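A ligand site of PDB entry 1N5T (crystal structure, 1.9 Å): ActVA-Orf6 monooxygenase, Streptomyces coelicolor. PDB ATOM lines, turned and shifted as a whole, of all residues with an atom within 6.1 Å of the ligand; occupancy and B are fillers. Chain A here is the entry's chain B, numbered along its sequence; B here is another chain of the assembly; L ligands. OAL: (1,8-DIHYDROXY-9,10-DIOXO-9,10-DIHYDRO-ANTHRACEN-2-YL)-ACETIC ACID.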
ATOM      1  N   ALA A  12       3.999  11.163  -7.163  1.00  0.00           N
ATOM      2  CA  ALA A  12       2.671  11.326  -7.804  1.00  0.00           C
ATOM      3  C   ALA A  12       1.635  10.947  -6.721  1.00  0.00           C
ATOM      4  O   ALA A  12       1.856  10.006  -5.926  1.00  0.00           O
ATOM      5  CB  ALA A  12       2.566  10.387  -9.010  1.00  0.00           C
ATOM      6  N   VAL A  14      -2.258   9.986  -6.757  1.00  0.00           N
ATOM      7  CA  VAL A  14      -3.277   9.587  -7.719  1.00  0.00           C
ATOM      8  C   VAL A  14      -4.542   9.246  -6.952  1.00  0.00           C
ATOM      9  O   VAL A  14      -4.464   8.437  -6.037  1.00  0.00           O
ATOM     10  CB  VAL A  14      -2.803   8.334  -8.508  1.00  0.00           C
ATOM     11  CG1 VAL A  14      -3.771   8.055  -9.666  1.00  0.00           C
ATOM     12  CG2 VAL A  14      -1.396   8.521  -9.050  1.00  0.00           C
ATOM     13  N   PHE A  16      -8.430   7.934  -7.036  1.00  0.00           N
ATOM     14  CA  PHE A  16      -9.437   7.183  -7.801  1.00  0.00           C
ATOM     15  C   PHE A  16     -10.800   7.292  -7.137  1.00  0.00           C
ATOM     16  O   PHE A  16     -10.918   6.799  -5.994  1.00  0.00           O
ATOM     17  CB  PHE A  16      -9.000   5.698  -7.753  1.00  0.00           C
ATOM     18  CG  PHE A  16      -7.667   5.336  -8.392  1.00  0.00           C
ATOM     19  CD1 PHE A  16      -6.483   5.483  -7.710  1.00  0.00           C
ATOM     20  CD2 PHE A  16      -7.645   4.830  -9.692  1.00  0.00           C
ATOM     21  CE1 PHE A  16      -5.253   5.160  -8.318  1.00  0.00           C
ATOM     22  CE2 PHE A  16      -6.426   4.482 -10.281  1.00  0.00           C
ATOM     23  CZ  PHE A  16      -5.255   4.632  -9.603  1.00  0.00           C
ATOM     24  N   ALA A  31      -4.589  -3.335  -7.679  1.00  0.00           N
ATOM     25  CA  ALA A  31      -3.310  -2.652  -7.875  1.00  0.00           C
ATOM     26  C   ALA A  31      -2.167  -3.267  -7.057  1.00  0.00           C
ATOM     27  O   ALA A  31      -0.987  -3.013  -7.331  1.00  0.00           O
ATOM     28  CB  ALA A  31      -3.442  -1.170  -7.513  1.00  0.00           C
ATOM     29  N   ILE A  39       6.454  -3.831 -11.284  1.00  0.00           N
ATOM     30  CA  ILE A  39       6.713  -2.437 -10.830  1.00  0.00           C
ATOM     31  C   ILE A  39       7.831  -2.317  -9.821  1.00  0.00           C
ATOM     32  O   ILE A  39       8.697  -1.410  -9.864  1.00  0.00           O
ATOM     33  CB  ILE A  39       5.395  -1.956 -10.150  1.00  0.00           C
ATOM     34  CG1 ILE A  39       4.337  -1.887 -11.251  1.00  0.00           C
ATOM     35  CG2 ILE A  39       5.587  -0.588  -9.546  1.00  0.00           C
ATOM     36  CD1 ILE A  39       2.923  -1.675 -10.695  1.00  0.00           C
ATOM     37  N   PHE A  45      11.891   3.348  -9.336  1.00  0.00           N
ATOM     38  CA  PHE A  45      10.680   3.211  -8.527  1.00  0.00           C
ATOM     39  C   PHE A  45      11.079   3.100  -7.063  1.00  0.00           C
ATOM     40  O   PHE A  45      11.990   2.308  -6.695  1.00  0.00           O
ATOM     41  CB  PHE A  45       9.877   1.983  -8.913  1.00  0.00           C
ATOM     42  CG  PHE A  45       8.745   1.586  -7.984  1.00  0.00           C
ATOM     43  CD1 PHE A  45       7.547   2.308  -7.944  1.00  0.00           C
ATOM     44  CD2 PHE A  45       8.911   0.511  -7.145  1.00  0.00           C
ATOM     45  CE1 PHE A  45       6.529   1.891  -7.100  1.00  0.00           C
ATOM     46  CE2 PHE A  45       7.908   0.128  -6.262  1.00  0.00           C
ATOM     47  CZ  PHE A  45       6.692   0.807  -6.260  1.00  0.00           C
ATOM     48  N   SER A  47       8.364   3.655  -4.249  1.00  0.00           N
ATOM     49  CA  SER A  47       7.258   3.052  -3.532  1.00  0.00           C
ATOM     50  C   SER A  47       5.906   3.485  -4.079  1.00  0.00           C
ATOM     51  O   SER A  47       5.899   4.490  -4.784  1.00  0.00           O
ATOM     52  CB  SER A  47       7.174   3.453  -2.040  1.00  0.00           C
ATOM     53  OG  SER A  47       6.894   4.891  -2.012  1.00  0.00           O
ATOM     54  N   ALA A  48       4.896   2.658  -3.786  1.00  0.00           N
ATOM     55  CA  ALA A  48       3.514   3.084  -4.064  1.00  0.00           C
ATOM     56  C   ALA A  48       2.661   2.657  -2.863  1.00  0.00           C
ATOM     57  O   ALA A  48       2.635   1.466  -2.474  1.00  0.00           O
ATOM     58  CB  ALA A  48       3.015   2.581  -5.386  1.00  0.00           C
ATOM     59  N   TYR A  50      -1.064   2.662  -1.245  1.00  0.00           N
ATOM     60  CA  TYR A  50      -2.473   2.864  -1.453  1.00  0.00           C
ATOM     61  C   TYR A  50      -3.214   3.030  -0.129  1.00  0.00           C
ATOM     62  O   TYR A  50      -2.949   2.346   0.871  1.00  0.00           O
ATOM     63  CB  TYR A  50      -3.037   1.641  -2.217  1.00  0.00           C
ATOM     64  CG  TYR A  50      -2.656   1.681  -3.685  1.00  0.00           C
ATOM     65  CD1 TYR A  50      -1.454   1.131  -4.126  1.00  0.00           C
ATOM     66  CD2 TYR A  50      -3.541   2.205  -4.612  1.00  0.00           C
ATOM     67  CE1 TYR A  50      -1.120   1.167  -5.469  1.00  0.00           C
ATOM     68  CE2 TYR A  50      -3.223   2.235  -5.956  1.00  0.00           C
ATOM     69  CZ  TYR A  50      -2.010   1.710  -6.357  1.00  0.00           C
ATOM     70  OH  TYR A  50      -1.716   1.744  -7.721  1.00  0.00           O
ATOM     71  N   ASN A  61      -3.184   6.845  -4.062  1.00  0.00           N
ATOM     72  CA  ASN A  61      -1.863   6.257  -4.081  1.00  0.00           C
ATOM     73  C   ASN A  61      -0.849   7.399  -3.917  1.00  0.00           C
ATOM     74  O   ASN A  61      -0.846   8.338  -4.737  1.00  0.00           O
ATOM     75  CB  ASN A  61      -1.674   5.558  -5.445  1.00  0.00           C
ATOM     76  CG  ASN A  61      -0.266   5.101  -5.768  1.00  0.00           C
ATOM     77  OD1 ASN A  61       0.573   4.988  -4.895  1.00  0.00           O
ATOM     78  ND2 ASN A  61       0.057   4.802  -7.040  1.00  0.00           N
ATOM     79  N   ALA A  63       2.943   7.904  -4.411  1.00  0.00           N
ATOM     80  CA  ALA A  63       4.007   7.078  -5.033  1.00  0.00           C
ATOM     81  C   ALA A  63       5.338   7.835  -5.082  1.00  0.00           C
ATOM     82  O   ALA A  63       5.357   9.000  -5.502  1.00  0.00           O
ATOM     83  CB  ALA A  63       3.540   6.726  -6.466  1.00  0.00           C
ATOM     84  N   GLN A  64       6.433   7.213  -4.684  1.00  0.00           N
ATOM     85  CA  GLN A  64       7.726   7.874  -4.628  1.00  0.00           C
ATOM     86  C   GLN A  64       8.641   7.387  -5.763  1.00  0.00           C
ATOM     87  O   GLN A  64       8.625   6.154  -6.012  1.00  0.00           O
ATOM     88  CB  GLN A  64       8.438   7.526  -3.324  1.00  0.00           C
ATOM     89  CG  GLN A  64       7.742   8.052  -2.055  1.00  0.00           C
ATOM     90  CD  GLN A  64       8.458   7.461  -0.855  1.00  0.00           C
ATOM     91  OE1 GLN A  64       8.686   6.237  -0.796  1.00  0.00           O
ATOM     92  NE2 GLN A  64       8.783   8.297   0.113  1.00  0.00           N
ATOM     93  N   TRP A  65       9.181   8.309  -6.548  1.00  0.00           N
ATOM     94  CA  TRP A  65      10.048   7.970  -7.661  1.00  0.00           C
ATOM     95  C   TRP A  65      11.386   8.738  -7.512  1.00  0.00           C
ATOM     96  O   TRP A  65      11.401   9.882  -6.991  1.00  0.00           O
ATOM     97  CB  TRP A  65       9.443   8.404  -8.996  1.00  0.00           C
ATOM     98  CG  TRP A  65       8.164   7.646  -9.277  1.00  0.00           C
ATOM     99  CD1 TRP A  65       6.932   7.944  -8.811  1.00  0.00           C
ATOM    100  CD2 TRP A  65       8.071   6.383  -9.953  1.00  0.00           C
ATOM    101  NE1 TRP A  65       6.048   6.992  -9.232  1.00  0.00           N
ATOM    102  CE2 TRP A  65       6.729   6.025  -9.957  1.00  0.00           C
ATOM    103  CE3 TRP A  65       8.983   5.572 -10.643  1.00  0.00           C
ATOM    104  CZ2 TRP A  65       6.245   4.858 -10.557  1.00  0.00           C
ATOM    105  CZ3 TRP A  65       8.503   4.440 -11.281  1.00  0.00           C
ATOM    106  CH2 TRP A  65       7.159   4.105 -11.224  1.00  0.00           C
ATOM    107  N   TYR A  71       9.308   7.889 -13.724  1.00  0.00           N
ATOM    108  CA  TYR A  71       7.893   7.683 -13.785  1.00  0.00           C
ATOM    109  C   TYR A  71       7.389   7.703 -15.231  1.00  0.00           C
ATOM    110  O   TYR A  71       6.632   6.774 -15.591  1.00  0.00           O
ATOM    111  CB  TYR A  71       7.169   8.844 -13.003  1.00  0.00           C
ATOM    112  CG  TYR A  71       5.688   8.827 -13.254  1.00  0.00           C
ATOM    113  CD1 TYR A  71       4.855   7.841 -12.698  1.00  0.00           C
ATOM    114  CD2 TYR A  71       5.110   9.826 -14.009  1.00  0.00           C
ATOM    115  CE1 TYR A  71       3.486   7.821 -12.950  1.00  0.00           C
ATOM    116  CE2 TYR A  71       3.737   9.843 -14.233  1.00  0.00           C
ATOM    117  CZ  TYR A  71       2.946   8.837 -13.717  1.00  0.00           C
ATOM    118  OH  TYR A  71       1.591   8.898 -13.963  1.00  0.00           O
ATOM    119  N   PHE A  75       8.551   3.571 -16.232  1.00  0.00           N
ATOM    120  CA  PHE A  75       7.251   3.020 -15.924  1.00  0.00           C
ATOM    121  C   PHE A  75       6.270   3.247 -17.071  1.00  0.00           C
ATOM    122  O   PHE A  75       5.746   2.291 -17.640  1.00  0.00           O
ATOM    123  CB  PHE A  75       6.706   3.645 -14.606  1.00  0.00           C
ATOM    124  CG  PHE A  75       5.328   3.189 -14.210  1.00  0.00           C
ATOM    125  CD1 PHE A  75       5.099   1.880 -13.837  1.00  0.00           C
ATOM    126  CD2 PHE A  75       4.273   4.092 -14.150  1.00  0.00           C
ATOM    127  CE1 PHE A  75       3.847   1.441 -13.414  1.00  0.00           C
ATOM    128  CE2 PHE A  75       3.009   3.683 -13.766  1.00  0.00           C
ATOM    129  CZ  PHE A  75       2.810   2.357 -13.377  1.00  0.00           C
ATOM    130  N   LEU A  84      -1.999  -2.091 -16.973  1.00  0.00           N
ATOM    131  CA  LEU A  84      -2.492  -1.811 -15.638  1.00  0.00           C
ATOM    132  C   LEU A  84      -3.478  -0.644 -15.651  1.00  0.00           C
ATOM    133  O   LEU A  84      -4.567  -0.754 -15.063  1.00  0.00           O
ATOM    134  CB  LEU A  84      -1.300  -1.428 -14.753  1.00  0.00           C
ATOM    135  CG  LEU A  84      -1.569  -0.859 -13.365  1.00  0.00           C
ATOM    136  CD1 LEU A  84      -2.343  -1.826 -12.478  1.00  0.00           C
ATOM    137  CD2 LEU A  84      -0.264  -0.416 -12.716  1.00  0.00           C
ATOM    138  N   ARG A  85      -3.135   0.443 -16.342  1.00  0.00           N
ATOM    139  CA  ARG A  85      -4.107   1.565 -16.401  1.00  0.00           C
ATOM    140  C   ARG A  85      -5.486   1.166 -16.881  1.00  0.00           C
ATOM    141  O   ARG A  85      -6.527   1.479 -16.288  1.00  0.00           O
ATOM    142  CB  ARG A  85      -3.398   2.696 -17.145  1.00  0.00           C
ATOM    143  CG  ARG A  85      -2.442   3.388 -16.147  1.00  0.00           C
ATOM    144  CD  ARG A  85      -1.330   4.156 -16.828  1.00  0.00           C
ATOM    145  NE  ARG A  85      -0.673   5.103 -15.953  1.00  0.00           N
ATOM    146  CZ  ARG A  85       0.448   5.789 -16.059  1.00  0.00           C
ATOM    147  NH1 ARG A  85       1.293   5.684 -17.091  1.00  0.00           N
ATOM    148  NH2 ARG A  85       0.770   6.628 -15.078  1.00  0.00           N
ATOM    149  N   LEU A  88      -7.520  -0.917 -14.254  1.00  0.00           N
ATOM    150  CA  LEU A  88      -7.982  -0.109 -13.127  1.00  0.00           C
ATOM    151  C   LEU A  88      -9.193   0.700 -13.576  1.00  0.00           C
ATOM    152  O   LEU A  88     -10.093   0.868 -12.768  1.00  0.00           O
ATOM    153  CB  LEU A  88      -6.892   0.839 -12.601  1.00  0.00           C
ATOM    154  CG  LEU A  88      -5.725   0.166 -11.883  1.00  0.00           C
ATOM    155  CD1 LEU A  88      -4.680   1.180 -11.432  1.00  0.00           C
ATOM    156  CD2 LEU A  88      -6.197  -0.674 -10.699  1.00  0.00           C
ATOM    157  N   PRO A  98      -9.158   8.402 -12.808  1.00  0.00           N
ATOM    158  CA  PRO A  98      -8.238   8.782 -11.771  1.00  0.00           C
ATOM    159  C   PRO A  98      -7.662  10.151 -12.080  1.00  0.00           C
ATOM    160  O   PRO A  98      -7.533  10.517 -13.258  1.00  0.00           O
ATOM    161  CB  PRO A  98      -7.064   7.786 -11.838  1.00  0.00           C
ATOM    162  CG  PRO A  98      -7.368   6.883 -12.963  1.00  0.00           C
ATOM    163  CD  PRO A  98      -8.752   7.158 -13.494  1.00  0.00           C
ATOM    164  N   LYS A  99      -7.317  10.888 -11.034  1.00  0.00           N
ATOM    165  CA  LYS A  99      -6.724  12.202 -11.260  1.00  0.00           C
ATOM    166  C   LYS A  99      -5.374  12.190 -10.510  1.00  0.00           C
ATOM    167  O   LYS A  99      -5.338  11.866  -9.342  1.00  0.00           O
ATOM    168  CB  LYS A  99      -7.576  13.346 -10.742  1.00  0.00           C
ATOM    169  CG  LYS A  99      -8.562  13.965 -11.732  1.00  0.00           C
ATOM    170  CD  LYS A  99      -9.762  13.138 -12.078  1.00  0.00           C
ATOM    171  CE  LYS A  99     -10.686  13.783 -13.107  1.00  0.00           C
ATOM    172  NZ  LYS A  99      -9.977  13.818 -14.441  1.00  0.00           N
ATOM    173  N   ALA A 100      -4.331  12.523 -11.241  1.00  0.00           N
ATOM    174  CA  ALA A 100      -3.020  12.548 -10.596  1.00  0.00           C
ATOM    175  C   ALA A 100      -2.593  13.990 -10.403  1.00  0.00           C
ATOM    176  O   ALA A 100      -2.867  14.892 -11.213  1.00  0.00           O
ATOM    177  CB  ALA A 100      -2.112  11.767 -11.545  1.00  0.00           C
ATOM    178  N   PHE A 102       1.250  15.847  -9.681  1.00  0.00           N
ATOM    179  CA  PHE A 102       2.690  15.524  -9.675  1.00  0.00           C
ATOM    180  C   PHE A 102       3.360  16.613  -8.816  1.00  0.00           C
ATOM    181  O   PHE A 102       2.899  17.751  -9.000  1.00  0.00           O
ATOM    182  CB  PHE A 102       3.189  15.541 -11.124  1.00  0.00           C
ATOM    183  CG  PHE A 102       2.473  14.438 -11.907  1.00  0.00           C
ATOM    184  CD1 PHE A 102       2.653  13.097 -11.512  1.00  0.00           C
ATOM    185  CD2 PHE A 102       1.595  14.733 -12.904  1.00  0.00           C
ATOM    186  CE1 PHE A 102       1.945  12.091 -12.154  1.00  0.00           C
ATOM    187  CE2 PHE A 102       0.912  13.688 -13.540  1.00  0.00           C
ATOM    188  CZ  PHE A 102       1.082  12.380 -13.221  1.00  0.00           C
ATOM    189  N   ILE B 109       3.443  -1.115  -2.290  1.00  0.00           N
ATOM    190  CA  ILE B 109       4.425  -1.884  -3.096  1.00  0.00           C
ATOM    191  C   ILE B 109       5.800  -1.275  -2.880  1.00  0.00           C
ATOM    192  O   ILE B 109       5.940  -0.064  -3.186  1.00  0.00           O
ATOM    193  CB  ILE B 109       4.044  -1.783  -4.584  1.00  0.00           C
ATOM    194  CG1 ILE B 109       2.629  -2.308  -4.878  1.00  0.00           C
ATOM    195  CG2 ILE B 109       5.088  -2.550  -5.393  1.00  0.00           C
ATOM    196  CD1 ILE B 109       2.205  -2.145  -6.337  1.00  0.00           C
HETATM  197  C1  OAL L   1       2.866   3.056  -8.950  1.00  0.00           C
HETATM  198  C2  OAL L   1       1.732   2.655  -9.599  1.00  0.00           C
HETATM  199  C3  OAL L   1       0.955   3.617 -10.323  1.00  0.00           C
HETATM  200  C4  OAL L   1       1.367   4.971 -10.348  1.00  0.00           C
HETATM  201  C5  OAL L   1       2.562   5.348  -9.667  1.00  0.00           C
HETATM  202  C6  OAL L   1       3.270   4.415  -8.970  1.00  0.00           C
HETATM  203  C7  OAL L   1       0.652   5.934 -11.075  1.00  0.00           C
HETATM  204  C8  OAL L   1      -0.515   5.559 -11.752  1.00  0.00           C
HETATM  205  C9  OAL L   1      -0.977   4.203 -11.706  1.00  0.00           C
HETATM  206  C10 OAL L   1      -0.216   3.261 -11.019  1.00  0.00           C
HETATM  207  C11 OAL L   1      -1.355   6.583 -12.302  1.00  0.00           C
HETATM  208  C12 OAL L   1      -2.603   6.261 -12.770  1.00  0.00           C
HETATM  209  C13 OAL L   1      -3.076   4.911 -12.705  1.00  0.00           C
HETATM  210  C14 OAL L   1      -2.296   3.912 -12.186  1.00  0.00           C
HETATM  211  C15 OAL L   1      -3.527   7.326 -13.360  1.00  0.00           C
HETATM  212  C16 OAL L   1      -2.858   8.287 -14.286  1.00  0.00           C
HETATM  213  O1  OAL L   1       2.957   6.698  -9.753  1.00  0.00           O
HETATM  214  O2  OAL L   1       1.063   7.070 -11.071  1.00  0.00           O
HETATM  215  O3  OAL L   1      -0.784   7.900 -12.371  1.00  0.00           O
HETATM  216  O5  OAL L   1      -1.863   8.350 -15.006  1.00  0.00           O
HETATM  217  O4  OAL L   1      -3.132   9.555 -14.718  1.00  0.00           O
HETATM  218  O6  OAL L   1      -0.570   2.078 -11.002  1.00  0.00           O
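An oxygen (O3) of the ligand lies within hydrogen-bond range of the side-chain hydroxyl (OH) of Tyr 71 (3.0 Å).
O5 of the ligand lies within salt-bridge range of NH2 of Arg 85 (3.1 Å).
NE1 of Trp 65 lies within hydrogen-bond range of O1 of the ligand.
An oxygen (O6) of the ligand is in hydrogen-bond range of the side-chain hydroxyl (OH) of Tyr 50.
The side-chain hydroxyl (OH) of Tyr 71 lies within hydrogen-bond range of the guanidinium group (NH2) of Arg 85 (2.7 Å).
The backbone NH (N) of Ala 63 sits at hydrogen-bond distance from the backbone carbonyl oxygen (O) of Ala 12, 2.8 Å away.
The backbone carbonyl oxygen (O) of Val 14 lies within hydrogen-bond range of the backbone NH (N) of Asn 61, 2.8 Å away.
O of Ala 48 sits at hydrogen-bond distance from N of Ile 109 of chain B (2.7 Å).
CB of Ala 12 touches O1 of the ligand, at 3.8 Å.
Val 14 touches the ligand.
CZ of Phe 16 touches C13 of the ligand, 3.8 Å away.
Ala 48 touches the ligand (CB to C1, 3.6 Å).
ND2 of Asn 61 touches C4 of the ligand, 3.6 Å away.
CB of Ala 63 touches O1 of the ligand (3.3 Å).
Phe 75 touches the ligand.
Leu 84 touches the ligand (CD2 to O6, 3.0 Å).
Leu 88 touches the ligand.
CB of Pro 98 touches C15 of the ligand (3.9 Å).
Hydrophobic or aromatic side chains that line the ligand: Ala 12, Val 14, Phe 16, Ala 48, Ala 63, Trp 65, Tyr 71, Phe 75, Leu 84, Leu 88 and Pro 98.
Within 4 Å of the ligand: Ala 12, Val 14, Phe 16, Ala 48, Tyr 50, Asn 61, Ala 63, Trp 65, Tyr 71, Phe 75, Leu 84, Arg 85, Leu 88 and Pro 98.
The nearest printed residue that does not touch the ligand is Ala 100 (4.0002 Å).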
